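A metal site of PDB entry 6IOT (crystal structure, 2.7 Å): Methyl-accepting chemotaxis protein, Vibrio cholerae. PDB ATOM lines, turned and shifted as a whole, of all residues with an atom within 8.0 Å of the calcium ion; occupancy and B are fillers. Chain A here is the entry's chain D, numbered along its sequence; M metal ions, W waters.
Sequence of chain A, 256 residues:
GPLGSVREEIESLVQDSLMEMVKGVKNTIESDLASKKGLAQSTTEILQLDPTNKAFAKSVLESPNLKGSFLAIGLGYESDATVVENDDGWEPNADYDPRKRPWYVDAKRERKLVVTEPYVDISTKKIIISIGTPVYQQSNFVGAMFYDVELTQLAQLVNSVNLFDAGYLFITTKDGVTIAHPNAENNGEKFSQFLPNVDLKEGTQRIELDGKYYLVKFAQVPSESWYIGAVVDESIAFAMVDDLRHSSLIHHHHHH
N of Gly 89 is in hydrogen-bond range of OD1 of Asp 87 (2.8 Å).
Within 4 Å of the calcium ion: Glu 85, Asp 87, Trp 90 and Glu 91.
The nearest printed residue that does not touch the calcium ion is Asp 88 (4.2 Å).
O of Asp 87 binds the calcium ion, 2.4 Å away.
The calcium ion is bound by the side-chain carboxylate (OE2) of Glu 85, at 2.4 Å.
OE2 of Glu 91 is bound to the calcium ion (2.5 Å).
Water W2 binds the calcium ion, 2.5 Å away.
The backbone carbonyl oxygen (O) of Trp 90 is bound to the calcium ion (2.6 Å).
The calcium ion is bound by water W1.
The calcium ion has six donor atoms within binding distance.
Slightly farther from the calcium ion lies OE1 of Glu 85 (3.1 Å).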
ATOM      1  N   LYS A  58      18.078 -10.314 -10.816  1.00  0.00           N
ATOM      2  CA  LYS A  58      18.021  -9.053 -10.087  1.00  0.00           C
ATOM      3  C   LYS A  58      17.550  -7.911 -10.985  1.00  0.00           C
ATOM      4  O   LYS A  58      16.813  -7.037 -10.544  1.00  0.00           O
ATOM      5  CB  LYS A  58      19.388  -8.721  -9.490  1.00  0.00           C
ATOM      6  CG  LYS A  58      19.441  -8.787  -7.977  1.00  0.00           C
ATOM      7  CD  LYS A  58      18.675  -7.634  -7.350  1.00  0.00           C
ATOM      8  CE  LYS A  58      18.976  -7.497  -5.864  1.00  0.00           C
ATOM      9  NZ  LYS A  58      20.403  -7.141  -5.603  1.00  0.00           N
ATOM     10  N   GLU A  62      14.011  -5.810 -10.294  1.00  0.00           N
ATOM     11  CA  GLU A  62      14.161  -4.400  -9.964  1.00  0.00           C
ATOM     12  C   GLU A  62      13.387  -3.526 -10.931  1.00  0.00           C
ATOM     13  O   GLU A  62      13.355  -2.299 -10.791  1.00  0.00           O
ATOM     14  CB  GLU A  62      15.636  -3.996  -9.945  1.00  0.00           C
ATOM     15  CG  GLU A  62      16.448  -4.560  -8.789  1.00  0.00           C
ATOM     16  CD  GLU A  62      15.852  -4.220  -7.440  1.00  0.00           C
ATOM     17  OE1 GLU A  62      15.294  -3.119  -7.282  1.00  0.00           O
ATOM     18  OE2 GLU A  62      15.967  -5.063  -6.517  1.00  0.00           O
ATOM     19  N   VAL A  84      17.848 -14.289  -4.184  1.00  0.00           N
ATOM     20  CA  VAL A  84      17.814 -13.045  -4.947  1.00  0.00           C
ATOM     21  C   VAL A  84      16.516 -12.323  -4.637  1.00  0.00           C
ATOM     22  O   VAL A  84      15.440 -12.899  -4.779  1.00  0.00           O
ATOM     23  CB  VAL A  84      17.936 -13.288  -6.467  1.00  0.00           C
ATOM     24  CG1 VAL A  84      17.682 -12.002  -7.231  1.00  0.00           C
ATOM     25  CG2 VAL A  84      19.300 -13.874  -6.804  1.00  0.00           C
ATOM     26  N   GLU A  85      16.605 -11.062  -4.218  1.00  0.00           N
ATOM     27  CA  GLU A  85      15.459 -10.372  -3.637  1.00  0.00           C
ATOM     28  C   GLU A  85      15.476  -8.855  -3.907  1.00  0.00           C
ATOM     29  O   GLU A  85      16.535  -8.250  -3.996  1.00  0.00           O
ATOM     30  CB  GLU A  85      15.410 -10.670  -2.138  1.00  0.00           C
ATOM     31  CG  GLU A  85      14.829  -9.575  -1.281  1.00  0.00           C
ATOM     32  CD  GLU A  85      15.895  -8.643  -0.770  1.00  0.00           C
ATOM     33  OE1 GLU A  85      17.073  -9.041  -0.734  1.00  0.00           O
ATOM     34  OE2 GLU A  85      15.554  -7.505  -0.417  1.00  0.00           O
ATOM     35  N   ASN A  86      14.297  -8.252  -4.045  1.00  0.00           N
ATOM     36  CA  ASN A  86      14.184  -6.851  -4.452  1.00  0.00           C
ATOM     37  C   ASN A  86      13.656  -5.878  -3.390  1.00  0.00           C
ATOM     38  O   ASN A  86      13.186  -4.796  -3.724  1.00  0.00           O
ATOM     39  CB  ASN A  86      13.288  -6.760  -5.697  1.00  0.00           C
ATOM     40  CG  ASN A  86      11.818  -6.976  -5.379  1.00  0.00           C
ATOM     41  OD1 ASN A  86      11.461  -7.590  -4.372  1.00  0.00           O
ATOM     42  ND2 ASN A  86      10.949  -6.460  -6.244  1.00  0.00           N
ATOM     43  N   ASP A  87      13.750  -6.256  -2.122  1.00  0.00           N
ATOM     44  CA  ASP A  87      13.247  -5.418  -1.039  1.00  0.00           C
ATOM     45  C   ASP A  87      14.359  -4.552  -0.445  1.00  0.00           C
ATOM     46  O   ASP A  87      15.244  -5.041   0.258  1.00  0.00           O
ATOM     47  CB  ASP A  87      12.613  -6.283   0.056  1.00  0.00           C
ATOM     48  CG  ASP A  87      11.723  -5.487   0.999  1.00  0.00           C
ATOM     49  OD1 ASP A  87      12.031  -4.305   1.282  1.00  0.00           O
ATOM     50  OD2 ASP A  87      10.696  -6.047   1.453  1.00  0.00           O
ATOM     51  N   ASP A  88      14.301  -3.245  -0.694  1.00  0.00           N
ATOM     52  CA  ASP A  88      15.318  -2.328  -0.188  1.00  0.00           C
ATOM     53  C   ASP A  88      15.312  -2.225   1.339  1.00  0.00           C
ATOM     54  O   ASP A  88      16.137  -1.522   1.924  1.00  0.00           O
ATOM     55  CB  ASP A  88      15.125  -0.940  -0.798  1.00  0.00           C
ATOM     56  CG  ASP A  88      15.435  -0.903  -2.283  1.00  0.00           C
ATOM     57  OD1 ASP A  88      16.501  -1.432  -2.679  1.00  0.00           O
ATOM     58  OD2 ASP A  88      14.618  -0.360  -3.049  1.00  0.00           O
ATOM     59  N   GLY A  89      14.395  -2.945   1.984  1.00  0.00           N
ATOM     60  CA  GLY A  89      14.298  -2.928   3.430  1.00  0.00           C
ATOM     61  C   GLY A  89      14.408  -4.299   4.083  1.00  0.00           C
ATOM     62  O   GLY A  89      14.153  -4.441   5.284  1.00  0.00           O
ATOM     63  N   TRP A  90      14.775  -5.308   3.307  1.00  0.00           N
ATOM     64  CA  TRP A  90      14.957  -6.649   3.864  1.00  0.00           C
ATOM     65  C   TRP A  90      16.168  -7.371   3.276  1.00  0.00           C
ATOM     66  O   TRP A  90      16.435  -7.292   2.076  1.00  0.00           O
ATOM     67  CB  TRP A  90      13.712  -7.512   3.643  1.00  0.00           C
ATOM     68  CG  TRP A  90      13.874  -8.930   4.145  1.00  0.00           C
ATOM     69  CD1 TRP A  90      13.892  -9.332   5.451  1.00  0.00           C
ATOM     70  CD2 TRP A  90      14.045 -10.107   3.359  1.00  0.00           C
ATOM     71  NE1 TRP A  90      14.060 -10.688   5.518  1.00  0.00           N
ATOM     72  CE2 TRP A  90      14.160 -11.192   4.245  1.00  0.00           C
ATOM     73  CE3 TRP A  90      14.115 -10.352   1.978  1.00  0.00           C
ATOM     74  CZ2 TRP A  90      14.343 -12.505   3.802  1.00  0.00           C
ATOM     75  CZ3 TRP A  90      14.297 -11.659   1.543  1.00  0.00           C
ATOM     76  CH2 TRP A  90      14.409 -12.719   2.460  1.00  0.00           C
ATOM     77  N   GLU A  91      16.894  -8.062   4.142  1.00  0.00           N
ATOM     78  CA  GLU A  91      17.944  -8.973   3.718  1.00  0.00           C
ATOM     79  C   GLU A  91      17.882 -10.216   4.601  1.00  0.00           C
ATOM     80  O   GLU A  91      17.582 -10.105   5.787  1.00  0.00           O
ATOM     81  CB  GLU A  91      19.328  -8.310   3.804  1.00  0.00           C
ATOM     82  CG  GLU A  91      19.595  -7.263   2.723  1.00  0.00           C
ATOM     83  CD  GLU A  91      19.758  -7.874   1.337  1.00  0.00           C
ATOM     84  OE1 GLU A  91      20.054  -9.083   1.244  1.00  0.00           O
ATOM     85  OE2 GLU A  91      19.597  -7.139   0.343  1.00  0.00           O
ATOM     86  N   PRO A  92      18.136 -11.394   4.016  1.00  0.00           N
ATOM     87  CA  PRO A  92      18.021 -12.678   4.721  1.00  0.00           C
ATOM     88  C   PRO A  92      18.803 -12.730   6.028  1.00  0.00           C
ATOM     89  O   PRO A  92      19.866 -12.140   6.158  1.00  0.00           O
ATOM     90  CB  PRO A  92      18.598 -13.679   3.724  1.00  0.00           C
ATOM     91  CG  PRO A  92      18.347 -13.060   2.391  1.00  0.00           C
ATOM     92  CD  PRO A  92      18.519 -11.583   2.604  1.00  0.00           C
HETATM   93 CA    CA M   1      17.403  -6.011   0.042  1.00  0.00          CA
HETATM   94  O   HOH W   1      18.578  -3.507   0.851  1.00  0.00           O
HETATM   95  O   HOH W   2      17.706  -6.536  -2.407  1.00  0.00           O
